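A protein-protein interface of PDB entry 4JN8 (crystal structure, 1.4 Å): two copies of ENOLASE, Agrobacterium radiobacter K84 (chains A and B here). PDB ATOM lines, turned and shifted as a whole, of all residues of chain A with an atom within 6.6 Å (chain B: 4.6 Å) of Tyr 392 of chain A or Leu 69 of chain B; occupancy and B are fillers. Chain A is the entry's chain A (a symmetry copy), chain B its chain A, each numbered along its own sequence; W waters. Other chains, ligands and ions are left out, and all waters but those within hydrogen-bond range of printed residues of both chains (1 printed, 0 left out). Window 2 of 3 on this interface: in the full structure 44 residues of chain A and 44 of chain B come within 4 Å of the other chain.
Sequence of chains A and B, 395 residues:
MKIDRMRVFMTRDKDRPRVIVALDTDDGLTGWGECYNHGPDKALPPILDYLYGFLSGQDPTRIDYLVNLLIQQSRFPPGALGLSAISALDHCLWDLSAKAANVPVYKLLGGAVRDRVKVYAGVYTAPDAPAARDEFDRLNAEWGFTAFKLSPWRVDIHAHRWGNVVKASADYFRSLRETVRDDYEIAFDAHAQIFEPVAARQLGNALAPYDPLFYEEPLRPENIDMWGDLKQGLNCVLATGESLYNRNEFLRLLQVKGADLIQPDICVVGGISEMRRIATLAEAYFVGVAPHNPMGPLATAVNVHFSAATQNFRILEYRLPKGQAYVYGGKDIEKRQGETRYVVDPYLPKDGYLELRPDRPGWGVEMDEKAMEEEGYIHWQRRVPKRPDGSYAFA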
ATOM      1  N   VAL A 384      -1.996  20.837 -19.573  1.00  0.00           N
ATOM      2  CA  VAL A 384      -3.278  21.493 -19.700  1.00  0.00           C
ATOM      3  C   VAL A 384      -3.075  22.692 -20.619  1.00  0.00           C
ATOM      4  O   VAL A 384      -2.313  23.597 -20.290  1.00  0.00           O
ATOM      5  CB  VAL A 384      -3.795  21.967 -18.349  1.00  0.00           C
ATOM      6  CG1 VAL A 384      -5.165  22.603 -18.509  1.00  0.00           C
ATOM      7  CG2 VAL A 384      -3.868  20.779 -17.376  1.00  0.00           C
ATOM      8  N   PRO A 385      -3.744  22.680 -21.761  1.00  0.00           N
ATOM      9  CA  PRO A 385      -3.505  23.784 -22.694  1.00  0.00           C
ATOM     10  C   PRO A 385      -4.093  25.087 -22.205  1.00  0.00           C
ATOM     11  O   PRO A 385      -5.022  25.106 -21.392  1.00  0.00           O
ATOM     12  CB  PRO A 385      -4.225  23.334 -23.953  1.00  0.00           C
ATOM     13  CG  PRO A 385      -5.300  22.444 -23.474  1.00  0.00           C
ATOM     14  CD  PRO A 385      -4.772  21.754 -22.252  1.00  0.00           C
ATOM     15  N   LYS A 386      -3.540  26.164 -22.728  1.00  0.00           N
ATOM     16  CA  LYS A 386      -3.965  27.505 -22.381  1.00  0.00           C
ATOM     17  C   LYS A 386      -4.565  28.182 -23.593  1.00  0.00           C
ATOM     18  O   LYS A 386      -4.271  27.852 -24.753  1.00  0.00           O
ATOM     19  CB  LYS A 386      -2.783  28.313 -21.878  1.00  0.00           C
ATOM     20  CG  LYS A 386      -2.024  27.579 -20.767  1.00  0.00           C
ATOM     21  CD  LYS A 386      -1.163  28.519 -19.991  1.00  0.00           C
ATOM     22  CE  LYS A 386      -2.007  29.307 -19.024  1.00  0.00           C
ATOM     23  NZ  LYS A 386      -1.182  30.238 -18.248  1.00  0.00           N
ATOM     24  N   ARG A 387      -5.423  29.149 -23.314  1.00  0.00           N
ATOM     25  CA  ARG A 387      -5.966  30.018 -24.334  1.00  0.00           C
ATOM     26  C   ARG A 387      -5.039  31.215 -24.485  1.00  0.00           C
ATOM     27  O   ARG A 387      -4.215  31.469 -23.617  1.00  0.00           O
ATOM     28  CB  ARG A 387      -7.361  30.496 -23.935  1.00  0.00           C
ATOM     29  CG  ARG A 387      -8.325  29.356 -23.597  1.00  0.00           C
ATOM     30  CD  ARG A 387      -9.731  29.876 -23.444  1.00  0.00           C
ATOM     31  NE  ARG A 387     -10.652  28.813 -23.038  1.00  0.00           N
ATOM     32  CZ  ARG A 387     -10.776  28.361 -21.792  1.00  0.00           C
ATOM     33  NH1 ARG A 387     -10.039  28.875 -20.824  1.00  0.00           N
ATOM     34  NH2 ARG A 387     -11.614  27.366 -21.517  1.00  0.00           N
ATOM     35  N   ASP A 389      -5.558  34.249 -23.928  1.00  0.00           N
ATOM     36  CA  ASP A 389      -5.699  35.213 -22.834  1.00  0.00           C
ATOM     37  C   ASP A 389      -5.013  34.779 -21.532  1.00  0.00           C
ATOM     38  O   ASP A 389      -5.101  35.502 -20.537  1.00  0.00           O
ATOM     39  CB  ASP A 389      -7.173  35.556 -22.573  1.00  0.00           C
ATOM     40  CG  ASP A 389      -7.984  34.373 -22.031  1.00  0.00           C
ATOM     41  OD1 ASP A 389      -7.389  33.288 -21.785  1.00  0.00           O
ATOM     42  OD2 ASP A 389      -9.223  34.527 -21.881  1.00  0.00           O
ATOM     43  N   GLY A 390      -4.352  33.618 -21.532  1.00  0.00           N
ATOM     44  CA  GLY A 390      -3.644  33.107 -20.366  1.00  0.00           C
ATOM     45  C   GLY A 390      -4.435  32.169 -19.467  1.00  0.00           C
ATOM     46  O   GLY A 390      -3.892  31.646 -18.490  1.00  0.00           O
ATOM     47  N   SER A 391      -5.701  31.947 -19.778  1.00  0.00           N
ATOM     48  CA  SER A 391      -6.507  31.023 -18.981  1.00  0.00           C
ATOM     49  C   SER A 391      -6.175  29.577 -19.349  1.00  0.00           C
ATOM     50  O   SER A 391      -5.707  29.298 -20.444  1.00  0.00           O
ATOM     51  CB  SER A 391      -8.001  31.278 -19.200  1.00  0.00           C
ATOM     52  OG  SER A 391      -8.373  31.161 -20.573  1.00  0.00           O
ATOM     53  N   TYR A 392      -6.403  28.673 -18.412  1.00  0.00           N
ATOM     54  CA  TYR A 392      -6.318  27.240 -18.682  1.00  0.00           C
ATOM     55  C   TYR A 392      -7.616  26.697 -19.221  1.00  0.00           C
ATOM     56  O   TYR A 392      -8.688  27.031 -18.740  1.00  0.00           O
ATOM     57  CB  TYR A 392      -5.970  26.468 -17.406  1.00  0.00           C
ATOM     58  CG  TYR A 392      -4.510  26.511 -17.060  1.00  0.00           C
ATOM     59  CD1 TYR A 392      -3.583  25.844 -17.851  1.00  0.00           C
ATOM     60  CD2 TYR A 392      -4.047  27.216 -15.962  1.00  0.00           C
ATOM     61  CE1 TYR A 392      -2.242  25.869 -17.553  1.00  0.00           C
ATOM     62  CE2 TYR A 392      -2.687  27.256 -15.665  1.00  0.00           C
ATOM     63  CZ  TYR A 392      -1.808  26.583 -16.467  1.00  0.00           C
ATOM     64  OH  TYR A 392      -0.445  26.603 -16.188  1.00  0.00           O
ATOM     65  N   ALA A 393      -7.497  25.818 -20.214  1.00  0.00           N
ATOM     66  CA  ALA A 393      -8.640  25.126 -20.783  1.00  0.00           C
ATOM     67  C   ALA A 393      -8.685  23.694 -20.255  1.00  0.00           C
ATOM     68  O   ALA A 393      -8.652  23.497 -19.048  1.00  0.00           O
ATOM     69  CB  ALA A 393      -8.567  25.185 -22.318  1.00  0.00           C
ATOM     70  N   PHE A 394      -8.738  22.702 -21.144  1.00  0.00           N
ATOM     71  CA  PHE A 394      -9.007  21.323 -20.742  1.00  0.00           C
ATOM     72  C   PHE A 394      -8.015  20.354 -21.352  1.00  0.00           C
ATOM     73  O   PHE A 394      -7.710  20.440 -22.544  1.00  0.00           O
ATOM     74  CB  PHE A 394     -10.438  20.973 -21.123  1.00  0.00           C
ATOM     75  CG  PHE A 394     -11.433  21.944 -20.574  1.00  0.00           C
ATOM     76  CD1 PHE A 394     -11.784  21.916 -19.228  1.00  0.00           C
ATOM     77  CD2 PHE A 394     -11.973  22.934 -21.368  1.00  0.00           C
ATOM     78  CE1 PHE A 394     -12.673  22.827 -18.704  1.00  0.00           C
ATOM     79  CE2 PHE A 394     -12.858  23.850 -20.829  1.00  0.00           C
ATOM     80  CZ  PHE A 394     -13.201  23.800 -19.506  1.00  0.00           C
ATOM     81  N   PHE B  54       2.575  21.698  -9.712  1.00  0.00           N
ATOM     82  CA  PHE B  54       1.781  22.681 -10.446  1.00  0.00           C
ATOM     83  C   PHE B  54       1.662  24.019  -9.704  1.00  0.00           C
ATOM     84  O   PHE B  54       1.156  24.998 -10.261  1.00  0.00           O
ATOM     85  CB  PHE B  54       0.364  22.133 -10.715  1.00  0.00           C
ATOM     86  CG  PHE B  54       0.351  20.880 -11.544  1.00  0.00           C
ATOM     87  CD1 PHE B  54       0.254  20.949 -12.921  1.00  0.00           C
ATOM     88  CD2 PHE B  54       0.432  19.642 -10.947  1.00  0.00           C
ATOM     89  CE1 PHE B  54       0.237  19.796 -13.689  1.00  0.00           C
ATOM     90  CE2 PHE B  54       0.428  18.485 -11.717  1.00  0.00           C
ATOM     91  CZ  PHE B  54       0.345  18.584 -13.088  1.00  0.00           C
ATOM     92  N   TYR B  65      -7.496  30.086 -10.204  1.00  0.00           N
ATOM     93  CA  TYR B  65      -6.640  29.732 -11.319  1.00  0.00           C
ATOM     94  C   TYR B  65      -5.852  28.472 -10.995  1.00  0.00           C
ATOM     95  O   TYR B  65      -5.770  27.540 -11.796  1.00  0.00           O
ATOM     96  CB  TYR B  65      -5.694  30.896 -11.537  1.00  0.00           C
ATOM     97  CG  TYR B  65      -4.627  30.751 -12.593  1.00  0.00           C
ATOM     98  CD1 TYR B  65      -4.946  30.746 -13.938  1.00  0.00           C
ATOM     99  CD2 TYR B  65      -3.280  30.678 -12.228  1.00  0.00           C
ATOM    100  CE1 TYR B  65      -3.932  30.677 -14.909  1.00  0.00           C
ATOM    101  CE2 TYR B  65      -2.284  30.607 -13.171  1.00  0.00           C
ATOM    102  CZ  TYR B  65      -2.610  30.602 -14.496  1.00  0.00           C
ATOM    103  OH  TYR B  65      -1.567  30.522 -15.415  1.00  0.00           O
ATOM    104  N   LEU B  66      -5.266  28.449  -9.811  1.00  0.00           N
ATOM    105  CA  LEU B  66      -4.435  27.333  -9.412  1.00  0.00           C
ATOM    106  C   LEU B  66      -5.257  26.097  -9.017  1.00  0.00           C
ATOM    107  O   LEU B  66      -4.890  24.962  -9.369  1.00  0.00           O
ATOM    108  CB  LEU B  66      -3.495  27.737  -8.286  1.00  0.00           C
ATOM    109  CG  LEU B  66      -2.464  28.802  -8.667  1.00  0.00           C
ATOM    110  CD1 LEU B  66      -1.704  29.263  -7.428  1.00  0.00           C
ATOM    111  CD2 LEU B  66      -1.513  28.296  -9.748  1.00  0.00           C
ATOM    112  N   VAL B  67      -6.349  26.299  -8.278  1.00  0.00           N
ATOM    113  CA  VAL B  67      -7.164  25.156  -7.893  1.00  0.00           C
ATOM    114  C   VAL B  67      -7.749  24.488  -9.146  1.00  0.00           C
ATOM    115  O   VAL B  67      -7.725  23.257  -9.280  1.00  0.00           O
ATOM    116  CB  VAL B  67      -8.253  25.535  -6.881  1.00  0.00           C
ATOM    117  CG1 VAL B  67      -9.116  24.332  -6.623  1.00  0.00           C
ATOM    118  CG2 VAL B  67      -7.620  26.030  -5.577  1.00  0.00           C
ATOM    119  N   ASN B  68      -8.208  25.287 -10.106  1.00  0.00           N
ATOM    120  CA  ASN B  68      -8.720  24.707 -11.337  1.00  0.00           C
ATOM    121  C   ASN B  68      -7.617  23.982 -12.104  1.00  0.00           C
ATOM    122  O   ASN B  68      -7.862  22.935 -12.707  1.00  0.00           O
ATOM    123  CB  ASN B  68      -9.404  25.775 -12.204  1.00  0.00           C
ATOM    124  CG  ASN B  68      -9.916  25.214 -13.510  1.00  0.00           C
ATOM    125  OD1 ASN B  68     -10.787  24.343 -13.524  1.00  0.00           O
ATOM    126  ND2 ASN B  68      -9.346  25.670 -14.607  1.00  0.00           N
ATOM    127  N   LEU B  69      -6.393  24.507 -12.091  1.00  0.00           N
ATOM    128  CA  LEU B  69      -5.290  23.782 -12.687  1.00  0.00           C
ATOM    129  C   LEU B  69      -5.114  22.403 -12.049  1.00  0.00           C
ATOM    130  O   LEU B  69      -4.938  21.403 -12.757  1.00  0.00           O
ATOM    131  CB  LEU B  69      -3.999  24.594 -12.589  1.00  0.00           C
ATOM    132  CG  LEU B  69      -2.732  23.892 -13.095  1.00  0.00           C
ATOM    133  CD1 LEU B  69      -2.859  23.452 -14.569  1.00  0.00           C
ATOM    134  CD2 LEU B  69      -1.530  24.799 -12.900  1.00  0.00           C
ATOM    135  N   LEU B  70      -5.166  22.342 -10.725  1.00  0.00           N
ATOM    136  CA  LEU B  70      -5.067  21.050 -10.042  1.00  0.00           C
ATOM    137  C   LEU B  70      -6.175  20.085 -10.449  1.00  0.00           C
ATOM    138  O   LEU B  70      -5.942  18.878 -10.597  1.00  0.00           O
ATOM    139  CB  LEU B  70      -5.085  21.233  -8.535  1.00  0.00           C
ATOM    140  CG  LEU B  70      -3.977  22.107  -7.934  1.00  0.00           C
ATOM    141  CD1 LEU B  70      -4.053  22.031  -6.431  1.00  0.00           C
ATOM    142  CD2 LEU B  70      -2.600  21.684  -8.462  1.00  0.00           C
ATOM    143  N   ILE B  71      -7.385  20.604 -10.633  1.00  0.00           N
ATOM    144  CA  ILE B  71      -8.487  19.778 -11.102  1.00  0.00           C
ATOM    145  C   ILE B  71      -8.274  19.326 -12.538  1.00  0.00           C
ATOM    146  O   ILE B  71      -8.446  18.143 -12.861  1.00  0.00           O
ATOM    147  CB  ILE B  71      -9.806  20.561 -11.015  1.00  0.00           C
ATOM    148  CG1 ILE B  71     -10.155  20.810  -9.554  1.00  0.00           C
ATOM    149  CG2 ILE B  71     -10.925  19.799 -11.715  1.00  0.00           C
ATOM    150  CD1 ILE B  71     -11.268  21.814  -9.339  1.00  0.00           C
ATOM    151  N   GLN B  72      -7.882  20.238 -13.412  1.00  0.00           N
ATOM    152  CA  GLN B  72      -7.785  19.897 -14.816  1.00  0.00           C
ATOM    153  C   GLN B  72      -6.633  18.961 -15.124  1.00  0.00           C
ATOM    154  O   GLN B  72      -6.717  18.171 -16.070  1.00  0.00           O
ATOM    155  CB  GLN B  72      -7.658  21.142 -15.701  1.00  0.00           C
ATOM    156  CG  GLN B  72      -8.847  22.088 -15.650  1.00  0.00           C
ATOM    157  CD  GLN B  72     -10.175  21.423 -15.937  1.00  0.00           C
ATOM    158  OE1 GLN B  72     -10.266  20.475 -16.738  1.00  0.00           O
ATOM    159  NE2 GLN B  72     -11.227  21.928 -15.305  1.00  0.00           N
ATOM    160  N   GLN B  73      -5.535  19.042 -14.384  1.00  0.00           N
ATOM    161  CA  GLN B  73      -4.391  18.211 -14.744  1.00  0.00           C
ATOM    162  C   GLN B  73      -4.676  16.721 -14.628  1.00  0.00           C
ATOM    163  O   GLN B  73      -4.022  15.916 -15.286  1.00  0.00           O
ATOM    164  CB  GLN B  73      -3.134  18.587 -13.974  1.00  0.00           C
ATOM    165  CG  GLN B  73      -3.227  18.499 -12.507  1.00  0.00           C
ATOM    166  CD  GLN B  73      -3.164  17.079 -11.992  1.00  0.00           C
ATOM    167  OE1 GLN B  73      -2.536  16.206 -12.599  1.00  0.00           O
ATOM    168  NE2 GLN B  73      -3.820  16.830 -10.867  1.00  0.00           N
HETATM  169  O   HOH W   1     -10.245  25.104 -17.364  1.00  0.00           O
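The side-chain hydroxyl of Tyr 65 of chain B sits at hydrogen-bond distance from the side-chain amino group of Lys 386 of chain A, 2.9 Å away.
The side-chain amide nitrogen (NE2) of Gln 72 of chain B is in hydrogen-bond range of the side-chain amide oxygen (OD1) of Asn 68 of chain B, 3.0 Å away. The backbone carbonyl oxygen (O) of Leu 70 of chain B is in hydrogen-bond range of the side-chain amide nitrogen (NE2) of Gln 73 of chain B, at 3.0 Å. The backbone carbonyl oxygen of Pro 385 of chain A sits at hydrogen-bond distance from the backbone NH of Ala 393 of chain A (2.8 Å). O of Gly 390 of chain A lies close to NZ of Lys 386 of chain A, at 3.1 Å. The guanidinium group (NH1) of Arg 387 of chain A is in hydrogen-bond range of the backbone carbonyl oxygen (O) of Tyr 392 of chain A, at 3.1 Å.
Val 384 of chain A touches Gln 73 of chain B. Gly 390 of chain A touches Tyr 65 of chain B. Tyr 392 of chain A touches Tyr 65 of chain B. CD1 of Leu 69 of chain B touches CZ of Tyr 392 of chain A, 3.8 Å away. Gln 72 of chain B touches Ala 393 of chain A. Phe 394 of chain A touches Gln 72 of chain B.
Tyr 392 of chain A touches just these residues of chain B: Tyr 65 (3.5 Å) and Leu 69 (3.8 Å). Printed residues of chain A within 4 Å of Leu 69 of chain B: Tyr 392. Of the printed residues of chain A, Gln 72 of chain B touches Ala 393 (3.7 Å) and Phe 394 (3.3 Å). Printed residues of chain B within 4 Å of Ala 393 of chain A: Gln 72 (3.7 Å). Of the printed residues of chain A, Tyr 65 of chain B touches Lys 386, Gly 390 and Tyr 392. Of the printed residues of chain B, Lys 386 of chain A touches Tyr 65 (2.9 Å). Pro 385 of chain A touches none of the printed residues of chain B. Leu 66 of chain B touches none of the printed residues of chain A. The nearest printed residue of chain A that does not touch Leu 69 of chain B is Val 384 of chain A (4.01 Å).
Of the 10 printed residues of chain B, 4 touch a printed residue of chain A. Hydrophobic or aromatic side chains of chain B within 4 Å of the printed part of chain A: Tyr 65 and Leu 69. Of the 10 printed residues of chain A, 6 touch a printed residue of chain B. Printed residues of chain A that touch a printed residue of chain B: Val 384, Lys 386, Gly 390, Tyr 392, Ala 393 and Phe 394. Hydrophobic or aromatic side chains of chain A within 4 Å of the printed part of chain B: Val 384, Tyr 392 and Phe 394. Among the printed residues, no Asp or Glu carboxylate lies within 4 Å of a Lys or Arg side-chain nitrogen of the other chain.
No position is printed for both chains.
Water W1 lies within hydrogen-bond range of O of Ala 393 of chain A (2.8 Å), O of Tyr 392 of chain A (2.8 Å) and ND2 of Asn 68 of chain B (3.0 Å).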
